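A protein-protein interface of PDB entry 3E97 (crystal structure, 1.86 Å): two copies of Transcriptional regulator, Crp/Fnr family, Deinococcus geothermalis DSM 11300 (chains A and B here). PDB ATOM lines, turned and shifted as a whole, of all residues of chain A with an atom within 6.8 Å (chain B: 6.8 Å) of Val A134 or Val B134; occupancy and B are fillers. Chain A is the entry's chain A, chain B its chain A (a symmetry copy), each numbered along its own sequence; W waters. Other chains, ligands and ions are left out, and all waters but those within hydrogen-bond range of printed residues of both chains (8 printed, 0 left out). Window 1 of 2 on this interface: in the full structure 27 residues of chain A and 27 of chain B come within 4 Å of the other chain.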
ATOM      1  N   ARG A  62     -23.196  17.839  -8.299  1.00  0.00           N
ATOM      2  CA  ARG A  62     -24.458  18.413  -8.742  1.00  0.00           C
ATOM      3  C   ARG A  62     -25.298  17.158  -8.971  1.00  0.00           C
ATOM      4  O   ARG A  62     -24.854  16.229  -9.666  1.00  0.00           O
ATOM      5  CB  ARG A  62     -24.387  19.256 -10.023  1.00  0.00           C
ATOM      6  CG  ARG A  62     -23.642  20.599  -9.911  1.00  0.00           C
ATOM      7  CD  ARG A  62     -24.502  21.748 -10.461  1.00  0.00           C
ATOM      8  NE  ARG A  62     -23.734  22.937 -10.864  1.00  0.00           N
ATOM      9  CZ  ARG A  62     -23.706  23.451 -12.100  1.00  0.00           C
ATOM     10  NH1 ARG A  62     -24.450  22.930 -13.068  1.00  0.00           N
ATOM     11  NH2 ARG A  62     -22.980  24.539 -12.355  1.00  0.00           N
ATOM     12  N   THR A  84     -17.925  31.195  -5.518  1.00  0.00           N
ATOM     13  CA  THR A  84     -18.296  31.601  -6.886  1.00  0.00           C
ATOM     14  C   THR A  84     -19.677  32.292  -6.879  1.00  0.00           C
ATOM     15  O   THR A  84     -20.138  32.728  -7.925  1.00  0.00           O
ATOM     16  CB  THR A  84     -18.259  30.364  -7.862  1.00  0.00           C
ATOM     17  OG1 THR A  84     -17.095  29.567  -7.600  1.00  0.00           O
ATOM     18  CG2 THR A  84     -18.235  30.761  -9.345  1.00  0.00           C
ATOM     19  N   GLN A  90     -25.928  33.909  -9.929  1.00  0.00           N
ATOM     20  CA  GLN A  90     -26.462  32.662 -10.470  1.00  0.00           C
ATOM     21  C   GLN A  90     -26.412  31.583  -9.405  1.00  0.00           C
ATOM     22  O   GLN A  90     -25.399  31.438  -8.727  1.00  0.00           O
ATOM     23  CB  GLN A  90     -25.601  32.218 -11.649  1.00  0.00           C
ATOM     24  CG  GLN A  90     -25.587  33.201 -12.823  1.00  0.00           C
ATOM     25  CD  GLN A  90     -24.417  32.985 -13.763  1.00  0.00           C
ATOM     26  OE1 GLN A  90     -23.415  32.370 -13.397  1.00  0.00           O
ATOM     27  NE2 GLN A  90     -24.529  33.515 -14.975  1.00  0.00           N
ATOM     28  N   MET A 129      -7.944  32.554  -8.057  1.00  0.00           N
ATOM     29  CA  MET A 129      -8.548  31.236  -7.830  1.00  0.00           C
ATOM     30  C   MET A 129      -9.552  30.904  -8.948  1.00  0.00           C
ATOM     31  O   MET A 129      -9.495  29.813  -9.535  1.00  0.00           O
ATOM     32  CB  MET A 129      -9.231  31.208  -6.461  1.00  0.00           C
ATOM     33  CG  MET A 129      -8.233  31.291  -5.310  1.00  0.00           C
ATOM     34  SD  MET A 129      -9.112  31.798  -3.628  1.00  0.00           S
ATOM     35  CE  MET A 129     -10.585  30.716  -3.815  1.00  0.00           C
ATOM     36  N   LEU A 130     -10.420  31.868  -9.263  1.00  0.00           N
ATOM     37  CA  LEU A 130     -11.429  31.723 -10.321  1.00  0.00           C
ATOM     38  C   LEU A 130     -10.801  31.518 -11.696  1.00  0.00           C
ATOM     39  O   LEU A 130     -11.270  30.671 -12.463  1.00  0.00           O
ATOM     40  CB  LEU A 130     -12.373  32.932 -10.317  1.00  0.00           C
ATOM     41  CG  LEU A 130     -13.312  33.110  -9.121  1.00  0.00           C
ATOM     42  CD1 LEU A 130     -14.083  34.434  -9.209  1.00  0.00           C
ATOM     43  CD2 LEU A 130     -14.300  31.963  -9.005  1.00  0.00           C
ATOM     44  N   ALA A 131      -9.730  32.272 -11.994  1.00  0.00           N
ATOM     45  CA  ALA A 131      -8.988  32.172 -13.262  1.00  0.00           C
ATOM     46  C   ALA A 131      -8.357  30.780 -13.418  1.00  0.00           C
ATOM     47  O   ALA A 131      -8.424  30.157 -14.486  1.00  0.00           O
ATOM     48  CB  ALA A 131      -7.924  33.252 -13.346  1.00  0.00           C
ATOM     49  N   ARG A 132      -7.762  30.276 -12.335  1.00  0.00           N
ATOM     50  CA  ARG A 132      -7.246  28.912 -12.328  1.00  0.00           C
ATOM     51  C   ARG A 132      -8.333  27.872 -12.532  1.00  0.00           C
ATOM     52  O   ARG A 132      -8.095  26.874 -13.221  1.00  0.00           O
ATOM     53  CB  ARG A 132      -6.460  28.638 -11.044  1.00  0.00           C
ATOM     54  CG  ARG A 132      -5.157  29.450 -10.955  1.00  0.00           C
ATOM     55  CD  ARG A 132      -4.246  28.936  -9.839  1.00  0.00           C
ATOM     56  NE  ARG A 132      -4.857  28.941  -8.509  1.00  0.00           N
ATOM     57  CZ  ARG A 132      -4.772  29.940  -7.616  1.00  0.00           C
ATOM     58  NH1 ARG A 132      -4.115  31.062  -7.883  1.00  0.00           N
ATOM     59  NH2 ARG A 132      -5.364  29.824  -6.437  1.00  0.00           N
ATOM     60  N   ARG A 133      -9.515  28.107 -11.963  1.00  0.00           N
ATOM     61  CA  ARG A 133     -10.649  27.196 -12.115  1.00  0.00           C
ATOM     62  C   ARG A 133     -11.136  27.200 -13.559  1.00  0.00           C
ATOM     63  O   ARG A 133     -11.427  26.149 -14.113  1.00  0.00           O
ATOM     64  CB  ARG A 133     -11.796  27.537 -11.150  1.00  0.00           C
ATOM     65  CG  ARG A 133     -12.890  26.477 -11.152  1.00  0.00           C
ATOM     66  CD  ARG A 133     -12.279  25.160 -10.701  1.00  0.00           C
ATOM     67  NE  ARG A 133     -13.163  24.008 -10.738  1.00  0.00           N
ATOM     68  CZ  ARG A 133     -12.771  22.790 -10.371  1.00  0.00           C
ATOM     69  NH1 ARG A 133     -11.515  22.580  -9.935  1.00  0.00           N
ATOM     70  NH2 ARG A 133     -13.628  21.775 -10.438  1.00  0.00           N
ATOM     71  N   VAL A 134     -11.183  28.367 -14.192  1.00  0.00           N
ATOM     72  CA  VAL A 134     -11.549  28.436 -15.624  1.00  0.00           C
ATOM     73  C   VAL A 134     -10.578  27.656 -16.495  1.00  0.00           C
ATOM     74  O   VAL A 134     -10.990  26.883 -17.368  1.00  0.00           O
ATOM     75  CB  VAL A 134     -11.662  29.927 -16.122  1.00  0.00           C
ATOM     76  CG1 VAL A 134     -11.740  29.990 -17.651  1.00  0.00           C
ATOM     77  CG2 VAL A 134     -12.882  30.636 -15.443  1.00  0.00           C
ATOM     78  N   THR A 135      -9.295  27.798 -16.228  1.00  0.00           N
ATOM     79  CA  THR A 135      -8.265  27.140 -17.000  1.00  0.00           C
ATOM     80  C   THR A 135      -8.418  25.618 -16.839  1.00  0.00           C
ATOM     81  O   THR A 135      -8.413  24.863 -17.824  1.00  0.00           O
ATOM     82  CB  THR A 135      -6.866  27.638 -16.595  1.00  0.00           C
ATOM     83  OG1 THR A 135      -6.827  29.066 -16.725  1.00  0.00           O
ATOM     84  CG2 THR A 135      -5.780  27.024 -17.479  1.00  0.00           C
ATOM     85  N   PHE A 136      -8.594  25.201 -15.594  1.00  0.00           N
ATOM     86  CA  PHE A 136      -8.805  23.803 -15.259  1.00  0.00           C
ATOM     87  C   PHE A 136     -10.037  23.208 -15.967  1.00  0.00           C
ATOM     88  O   PHE A 136      -9.964  22.120 -16.524  1.00  0.00           O
ATOM     89  CB  PHE A 136      -8.925  23.652 -13.742  1.00  0.00           C
ATOM     90  CG  PHE A 136      -9.190  22.234 -13.308  1.00  0.00           C
ATOM     91  CD1 PHE A 136      -8.152  21.343 -13.162  1.00  0.00           C
ATOM     92  CD2 PHE A 136     -10.480  21.789 -13.120  1.00  0.00           C
ATOM     93  CE1 PHE A 136      -8.407  20.024 -12.800  1.00  0.00           C
ATOM     94  CE2 PHE A 136     -10.730  20.479 -12.775  1.00  0.00           C
ATOM     95  CZ  PHE A 136      -9.679  19.609 -12.619  1.00  0.00           C
ATOM     96  N   LEU A 137     -11.160  23.910 -15.928  1.00  0.00           N
ATOM     97  CA  LEU A 137     -12.393  23.425 -16.537  1.00  0.00           C
ATOM     98  C   LEU A 137     -12.282  23.358 -18.060  1.00  0.00           C
ATOM     99  O   LEU A 137     -12.866  22.461 -18.680  1.00  0.00           O
ATOM    100  CB  LEU A 137     -13.596  24.249 -16.067  1.00  0.00           C
ATOM    101  CG  LEU A 137     -13.985  24.114 -14.577  1.00  0.00           C
ATOM    102  CD1 LEU A 137     -15.041  25.170 -14.263  1.00  0.00           C
ATOM    103  CD2 LEU A 137     -14.475  22.671 -14.215  1.00  0.00           C
ATOM    104  N   ASN A 138     -11.530  24.282 -18.663  1.00  0.00           N
ATOM    105  CA  ASN A 138     -11.298  24.223 -20.119  1.00  0.00           C
ATOM    106  C   ASN A 138     -10.464  22.961 -20.425  1.00  0.00           C
ATOM    107  O   ASN A 138     -10.760  22.220 -21.364  1.00  0.00           O
ATOM    108  CB  ASN A 138     -10.607  25.501 -20.613  1.00  0.00           C
ATOM    109  CG  ASN A 138     -11.585  26.696 -20.733  1.00  0.00           C
ATOM    110  OD1 ASN A 138     -12.735  26.522 -21.079  1.00  0.00           O
ATOM    111  ND2 ASN A 138     -11.076  27.902 -20.526  1.00  0.00           N
ATOM    112  N   ASP A 139      -9.434  22.715 -19.621  1.00  0.00           N
ATOM    113  CA  ASP A 139      -8.615  21.508 -19.741  1.00  0.00           C
ATOM    114  C   ASP A 139      -9.486  20.265 -19.592  1.00  0.00           C
ATOM    115  O   ASP A 139      -9.354  19.317 -20.358  1.00  0.00           O
ATOM    116  CB  ASP A 139      -7.546  21.420 -18.649  1.00  0.00           C
ATOM    117  CG  ASP A 139      -6.435  22.432 -18.787  1.00  0.00           C
ATOM    118  OD1 ASP A 139      -6.303  23.045 -19.853  1.00  0.00           O
ATOM    119  OD2 ASP A 139      -5.667  22.572 -17.806  1.00  0.00           O
ATOM    120  N   GLU A 140     -10.382  20.285 -18.614  1.00  0.00           N
ATOM    121  CA  GLU A 140     -11.301  19.149 -18.384  1.00  0.00           C
ATOM    122  C   GLU A 140     -12.233  18.869 -19.575  1.00  0.00           C
ATOM    123  O   GLU A 140     -12.421  17.694 -20.008  1.00  0.00           O
ATOM    124  CB  GLU A 140     -12.089  19.371 -17.079  1.00  0.00           C
ATOM    125  CG  GLU A 140     -12.932  18.178 -16.706  1.00  0.00           C
ATOM    126  CD  GLU A 140     -13.240  18.042 -15.244  1.00  0.00           C
ATOM    127  OE1 GLU A 140     -12.307  18.073 -14.450  1.00  0.00           O
ATOM    128  OE2 GLU A 140     -14.422  17.851 -14.891  1.00  0.00           O
ATOM    129  N   ARG B  62      -8.926  25.640 -29.048  1.00  0.00           N
ATOM    130  CA  ARG B  62      -7.665  25.061 -28.607  1.00  0.00           C
ATOM    131  C   ARG B  62      -7.435  23.991 -29.671  1.00  0.00           C
ATOM    132  O   ARG B  62      -8.334  23.178 -29.945  1.00  0.00           O
ATOM    133  CB  ARG B  62      -7.680  24.435 -27.206  1.00  0.00           C
ATOM    134  CG  ARG B  62      -7.816  25.415 -26.025  1.00  0.00           C
ATOM    135  CD  ARG B  62      -6.721  25.163 -24.977  1.00  0.00           C
ATOM    136  NE  ARG B  62      -7.046  25.667 -23.633  1.00  0.00           N
ATOM    137  CZ  ARG B  62      -7.136  24.911 -22.531  1.00  0.00           C
ATOM    138  NH1 ARG B  62      -6.869  23.612 -22.575  1.00  0.00           N
ATOM    139  NH2 ARG B  62      -7.431  25.473 -21.359  1.00  0.00           N
ATOM    140  N   THR B  84      -8.006  35.919 -18.685  1.00  0.00           N
ATOM    141  CA  THR B  84      -7.807  34.857 -17.682  1.00  0.00           C
ATOM    142  C   THR B  84      -6.299  34.650 -17.420  1.00  0.00           C
ATOM    143  O   THR B  84      -5.939  33.827 -16.589  1.00  0.00           O
ATOM    144  CB  THR B  84      -8.517  33.525 -18.135  1.00  0.00           C
ATOM    145  OG1 THR B  84      -9.812  33.819 -18.677  1.00  0.00           O
ATOM    146  CG2 THR B  84      -8.701  32.516 -16.992  1.00  0.00           C
ATOM    147  N   GLN B  90      -0.701  30.541 -15.756  1.00  0.00           N
ATOM    148  CA  GLN B  90      -0.808  29.339 -16.577  1.00  0.00           C
ATOM    149  C   GLN B  90      -1.039  29.730 -18.024  1.00  0.00           C
ATOM    150  O   GLN B  90      -1.862  30.597 -18.301  1.00  0.00           O
ATOM    151  CB  GLN B  90      -2.001  28.513 -16.103  1.00  0.00           C
ATOM    152  CG  GLN B  90      -1.889  28.015 -14.660  1.00  0.00           C
ATOM    153  CD  GLN B  90      -3.223  27.604 -14.069  1.00  0.00           C
ATOM    154  OE1 GLN B  90      -4.282  28.002 -14.555  1.00  0.00           O
ATOM    155  NE2 GLN B  90      -3.177  26.822 -12.997  1.00  0.00           N
ATOM    156  N   MET B 129     -17.013  38.278 -14.079  1.00  0.00           N
ATOM    157  CA  MET B 129     -16.922  37.637 -15.395  1.00  0.00           C
ATOM    158  C   MET B 129     -16.381  36.203 -15.260  1.00  0.00           C
ATOM    159  O   MET B 129     -16.971  35.258 -15.804  1.00  0.00           O
ATOM    160  CB  MET B 129     -16.028  38.470 -16.317  1.00  0.00           C
ATOM    161  CG  MET B 129     -16.652  39.815 -16.673  1.00  0.00           C
ATOM    162  SD  MET B 129     -15.312  41.068 -17.376  1.00  0.00           S
ATOM    163  CE  MET B 129     -14.438  39.868 -18.458  1.00  0.00           C
ATOM    164  N   LEU B 130     -15.300  36.053 -14.491  1.00  0.00           N
ATOM    165  CA  LEU B 130     -14.670  34.750 -14.238  1.00  0.00           C
ATOM    166  C   LEU B 130     -15.604  33.786 -13.513  1.00  0.00           C
ATOM    167  O   LEU B 130     -15.665  32.606 -13.873  1.00  0.00           O
ATOM    168  CB  LEU B 130     -13.359  34.941 -13.464  1.00  0.00           C
ATOM    169  CG  LEU B 130     -12.193  35.629 -14.178  1.00  0.00           C
ATOM    170  CD1 LEU B 130     -11.014  35.864 -13.224  1.00  0.00           C
ATOM    171  CD2 LEU B 130     -11.715  34.829 -15.377  1.00  0.00           C
ATOM    172  N   ALA B 131     -16.345  34.294 -12.514  1.00  0.00           N
ATOM    173  CA  ALA B 131     -17.319  33.507 -11.739  1.00  0.00           C
ATOM    174  C   ALA B 131     -18.450  32.993 -12.644  1.00  0.00           C
ATOM    175  O   ALA B 131     -18.851  31.823 -12.572  1.00  0.00           O
ATOM    176  CB  ALA B 131     -17.884  34.332 -10.596  1.00  0.00           C
ATOM    177  N   ARG B 132     -18.947  33.865 -13.521  1.00  0.00           N
ATOM    178  CA  ARG B 132     -19.929  33.452 -14.517  1.00  0.00           C
ATOM    179  C   ARG B 132     -19.389  32.404 -15.473  1.00  0.00           C
ATOM    180  O   ARG B 132     -20.129  31.487 -15.850  1.00  0.00           O
ATOM    181  CB  ARG B 132     -20.469  34.663 -15.280  1.00  0.00           C
ATOM    182  CG  ARG B 132     -21.315  35.597 -14.397  1.00  0.00           C
ATOM    183  CD  ARG B 132     -22.095  36.612 -15.235  1.00  0.00           C
ATOM    184  NE  ARG B 132     -21.262  37.455 -16.094  1.00  0.00           N
ATOM    185  CZ  ARG B 132     -20.770  38.659 -15.761  1.00  0.00           C
ATOM    186  NH1 ARG B 132     -20.991  39.200 -14.569  1.00  0.00           N
ATOM    187  NH2 ARG B 132     -20.032  39.334 -16.629  1.00  0.00           N
ATOM    188  N   ARG B 133     -18.115  32.520 -15.848  1.00  0.00           N
ATOM    189  CA  ARG B 133     -17.473  31.554 -16.739  1.00  0.00           C
ATOM    190  C   ARG B 133     -17.338  30.206 -16.043  1.00  0.00           C
ATOM    191  O   ARG B 133     -17.593  29.173 -16.647  1.00  0.00           O
ATOM    192  CB  ARG B 133     -16.107  32.052 -17.238  1.00  0.00           C
ATOM    193  CG  ARG B 133     -15.525  31.156 -18.324  1.00  0.00           C
ATOM    194  CD  ARG B 133     -16.480  31.157 -19.506  1.00  0.00           C
ATOM    195  NE  ARG B 133     -16.130  30.271 -20.603  1.00  0.00           N
ATOM    196  CZ  ARG B 133     -16.868  30.166 -21.705  1.00  0.00           C
ATOM    197  NH1 ARG B 133     -17.987  30.901 -21.850  1.00  0.00           N
ATOM    198  NH2 ARG B 133     -16.497  29.328 -22.669  1.00  0.00           N
ATOM    199  N   VAL B 134     -16.986  30.204 -14.762  1.00  0.00           N
ATOM    200  CA  VAL B 134     -16.933  28.940 -13.995  1.00  0.00           C
ATOM    201  C   VAL B 134     -18.288  28.254 -13.938  1.00  0.00           C
ATOM    202  O   VAL B 134     -18.395  27.044 -14.169  1.00  0.00           O
ATOM    203  CB  VAL B 134     -16.369  29.169 -12.541  1.00  0.00           C
ATOM    204  CG1 VAL B 134     -16.598  27.933 -11.663  1.00  0.00           C
ATOM    205  CG2 VAL B 134     -14.858  29.573 -12.600  1.00  0.00           C
ATOM    206  N   THR B 135     -19.333  29.021 -13.700  1.00  0.00           N
ATOM    207  CA  THR B 135     -20.674  28.493 -13.587  1.00  0.00           C
ATOM    208  C   THR B 135     -21.080  27.877 -14.938  1.00  0.00           C
ATOM    209  O   THR B 135     -21.580  26.743 -15.003  1.00  0.00           O
ATOM    210  CB  THR B 135     -21.658  29.576 -13.113  1.00  0.00           C
ATOM    211  OG1 THR B 135     -21.177  30.131 -11.881  1.00  0.00           O
ATOM    212  CG2 THR B 135     -23.056  28.999 -12.893  1.00  0.00           C
ATOM    213  N   PHE B 136     -20.817  28.627 -15.998  1.00  0.00           N
ATOM    214  CA  PHE B 136     -21.088  28.186 -17.355  1.00  0.00           C
ATOM    215  C   PHE B 136     -20.354  26.877 -17.706  1.00  0.00           C
ATOM    216  O   PHE B 136     -20.951  25.964 -18.261  1.00  0.00           O
ATOM    217  CB  PHE B 136     -20.716  29.296 -18.339  1.00  0.00           C
ATOM    218  CG  PHE B 136     -20.925  28.906 -19.779  1.00  0.00           C
ATOM    219  CD1 PHE B 136     -22.167  29.017 -20.359  1.00  0.00           C
ATOM    220  CD2 PHE B 136     -19.893  28.367 -20.515  1.00  0.00           C
ATOM    221  CE1 PHE B 136     -22.363  28.616 -21.676  1.00  0.00           C
ATOM    222  CE2 PHE B 136     -20.093  27.958 -21.815  1.00  0.00           C
ATOM    223  CZ  PHE B 136     -21.337  28.091 -22.381  1.00  0.00           C
ATOM    224  N   LEU B 137     -19.068  26.799 -17.398  1.00  0.00           N
ATOM    225  CA  LEU B 137     -18.272  25.619 -17.715  1.00  0.00           C
ATOM    226  C   LEU B 137     -18.719  24.402 -16.906  1.00  0.00           C
ATOM    227  O   LEU B 137     -18.665  23.275 -17.411  1.00  0.00           O
ATOM    228  CB  LEU B 137     -16.776  25.914 -17.563  1.00  0.00           C
ATOM    229  CG  LEU B 137     -16.161  26.907 -18.575  1.00  0.00           C
ATOM    230  CD1 LEU B 137     -14.743  27.236 -18.119  1.00  0.00           C
ATOM    231  CD2 LEU B 137     -16.192  26.361 -20.043  1.00  0.00           C
ATOM    232  N   ASN B 138     -19.171  24.619 -15.669  1.00  0.00           N
ATOM    233  CA  ASN B 138     -19.711  23.505 -14.865  1.00  0.00           C
ATOM    234  C   ASN B 138     -21.006  23.005 -15.539  1.00  0.00           C
ATOM    235  O   ASN B 138     -21.220  21.800 -15.681  1.00  0.00           O
ATOM    236  CB  ASN B 138     -19.952  23.946 -13.415  1.00  0.00           C
ATOM    237  CG  ASN B 138     -18.642  24.017 -12.591  1.00  0.00           C
ATOM    238  OD1 ASN B 138     -17.746  23.222 -12.784  1.00  0.00           O
ATOM    239  ND2 ASN B 138     -18.598  24.922 -11.624  1.00  0.00           N
ATOM    240  N   ASP B 139     -21.857  23.935 -15.962  1.00  0.00           N
ATOM    241  CA  ASP B 139     -23.079  23.604 -16.698  1.00  0.00           C
ATOM    242  C   ASP B 139     -22.736  22.832 -17.967  1.00  0.00           C
ATOM    243  O   ASP B 139     -23.378  21.836 -18.282  1.00  0.00           O
ATOM    244  CB  ASP B 139     -23.844  24.852 -17.145  1.00  0.00           C
ATOM    245  CG  ASP B 139     -24.489  25.620 -16.017  1.00  0.00           C
ATOM    246  OD1 ASP B 139     -24.600  25.087 -14.906  1.00  0.00           O
ATOM    247  OD2 ASP B 139     -24.920  26.768 -16.282  1.00  0.00           O
ATOM    248  N   GLU B 140     -21.715  23.290 -18.680  1.00  0.00           N
ATOM    249  CA  GLU B 140     -21.270  22.613 -19.918  1.00  0.00           C
ATOM    250  C   GLU B 140     -20.790  21.171 -19.684  1.00  0.00           C
ATOM    251  O   GLU B 140     -21.159  20.220 -20.434  1.00  0.00           O
ATOM    252  CB  GLU B 140     -20.201  23.467 -20.624  1.00  0.00           C
ATOM    253  CG  GLU B 140     -19.816  22.909 -21.971  1.00  0.00           C
ATOM    254  CD  GLU B 140     -19.282  23.911 -22.951  1.00  0.00           C
ATOM    255  OE1 GLU B 140     -19.942  24.921 -23.167  1.00  0.00           O
ATOM    256  OE2 GLU B 140     -18.215  23.660 -23.551  1.00  0.00           O
HETATM  257  O   HOH W   1     -20.871  26.335 -10.744  1.00  0.00           O
HETATM  258  O   HOH W   2     -13.112  30.092 -21.026  1.00  0.00           O
HETATM  259  O   HOH W   3      -8.306  28.386 -20.350  1.00  0.00           O
HETATM  260  O   HOH W   4      -5.609  25.687 -13.577  1.00  0.00           O
HETATM  261  O   HOH W   5     -16.038  24.733 -10.011  1.00  0.00           O
HETATM  262  O   HOH W   6     -22.893  31.609 -16.086  1.00  0.00           O
HETATM  263  O   HOH W   7     -16.104  21.651 -11.458  1.00  0.00           O
HETATM  264  O   HOH W   8     -14.530  27.507 -22.730  1.00  0.00           O
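Water W7 lies within hydrogen-bond range of OD1 of Asn B138 (2.6 Å) and NH2 of Arg A133 (2.7 Å).
Water W8 bridges the side-chain amide oxygen of Asn A138 (2.6 Å) and the guanidinium group of Arg B133 (2.7 Å).
Water W4 lies within hydrogen-bond range of the side-chain amide nitrogen (NE2) of Gln B90 (2.7 Å) and the backbone carbonyl oxygen (O) of Arg A132 (2.8 Å).
Water W3 lies within hydrogen-bond range of the side-chain amide nitrogen of Asn A138 and the guanidinium group of Arg B62.
Water W5 bridges the side-chain amide nitrogen (ND2) of Asn B138 (3.0 Å) and the guanidinium group (NE) of Arg A133 (3.1 Å).
Water W2 bridges ND2 of Asn A138 (3.0 Å) and NE of Arg B133 (3.1 Å).
The backbone carbonyl oxygen of Ala A131 lies within hydrogen-bond range of the side-chain hydroxyl of Thr A135 (3.0 Å).
O of Val A134 lies within hydrogen-bond range of ND2 of Asn A138, at 3.3 Å.
O of Ala B131 sits at hydrogen-bond distance from OG1 of Thr B135 (3.0 Å).
The backbone carbonyl oxygen of Val B134 is in hydrogen-bond range of the side-chain amide nitrogen of Asn B138, 3.3 Å away.
Arg A62 touches Asn B138, and with the chains exchanged Asn A138 touches Arg B62.
Thr A84 touches Thr B135, and with the chains exchanged Thr A135 touches Thr B84.
Gln A90 touches Thr B135, and with the chains exchanged Thr A135 touches Gln B90.
Leu A130 touches its own counterpart, Leu B130.
15 positions are printed for both chains.
Among the printed residues, pairs that only touch across the chains: Arg A62 with Thr B135 (3.7 Å), Arg A62 with Asn B138 (3.3 Å), Thr A84 with Ala B131 (3.5 Å), Thr A84 with Thr B135 (3.9 Å), Gln A90 with Arg B132 (3.8 Å), Gln A90 with Thr B135 (3.3 Å), Leu A130 with Leu B130 (3.9 Å), Leu A130 with Val B134 (3.8 Å), Ala A131 with Thr B84 (3.5 Å), Arg A132 with Gln B90 (3.8 Å), Arg A133 with Val B134 (3.9 Å), Val A134 with Leu B130 (3.8 Å), Val A134 with Arg B133 (3.9 Å), Val A134 with Val B134 (3.6 Å), Val A134 with Leu B137 (3.8 Å), Thr A135 with Arg B62 (3.7 Å), Thr A135 with Thr B84 (3.9 Å), Thr A135 with Gln B90 (3.3 Å), Leu A137 with Val B134 (3.8 Å), Leu A137 with Leu B137 (3.8 Å), Leu A137 with Asn B138 (3.6 Å), Asn A138 with Arg B62 (3.3 Å) and Asn A138 with Leu B137 (3.6 Å).
The guanidinium group (NH1) of Arg A62 lies within salt-bridge range of the side-chain carboxylate (OD1) of Asp B139 (2.8 Å).
The guanidinium group (NH1) of Arg B62 lies within salt-bridge range of the side-chain carboxylate (OD1) of Asp A139.
Of the printed residues of chain B, Val A134 touches Leu B130, Arg B133, Val B134 and Leu B137.
Printed residues of chain A within 4 Å of Val B134: Leu A130 (3.8 Å), Arg A133 (3.9 Å), Val A134 (3.6 Å) and Leu A137 (3.8 Å).
Printed residues of chain A within 4 Å of Thr B135: Arg A62 (3.7 Å), Thr A84 (3.9 Å) and Gln A90 (3.3 Å).
Of the printed residues of chain B, Arg A133 touches Val B134 (3.9 Å).
Of the printed residues of chain A, Gln B90 touches Arg A132 and Thr A135.
Of the printed residues of chain B, Ala A131 touches Thr B84.
Of the printed residues of chain A, Asp B139 touches Arg A62.
The nearest printed residue of chain B that does not touch Val A134 is Thr B84 (4.01 Å).
The nearest printed residue of chain A that does not touch Val B134 is Thr A84 (4.01 Å).
The nearest printed residue of chain B that does not touch Thr A84 is Val B134 (4.01 Å).
Of the 15 printed residues of chain A, 12 touch a printed residue of chain B.
Hydrophobic or aromatic side chains of chain A that line the printed part of chain B: Leu A130, Ala A131, Val A134 and Leu A137.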
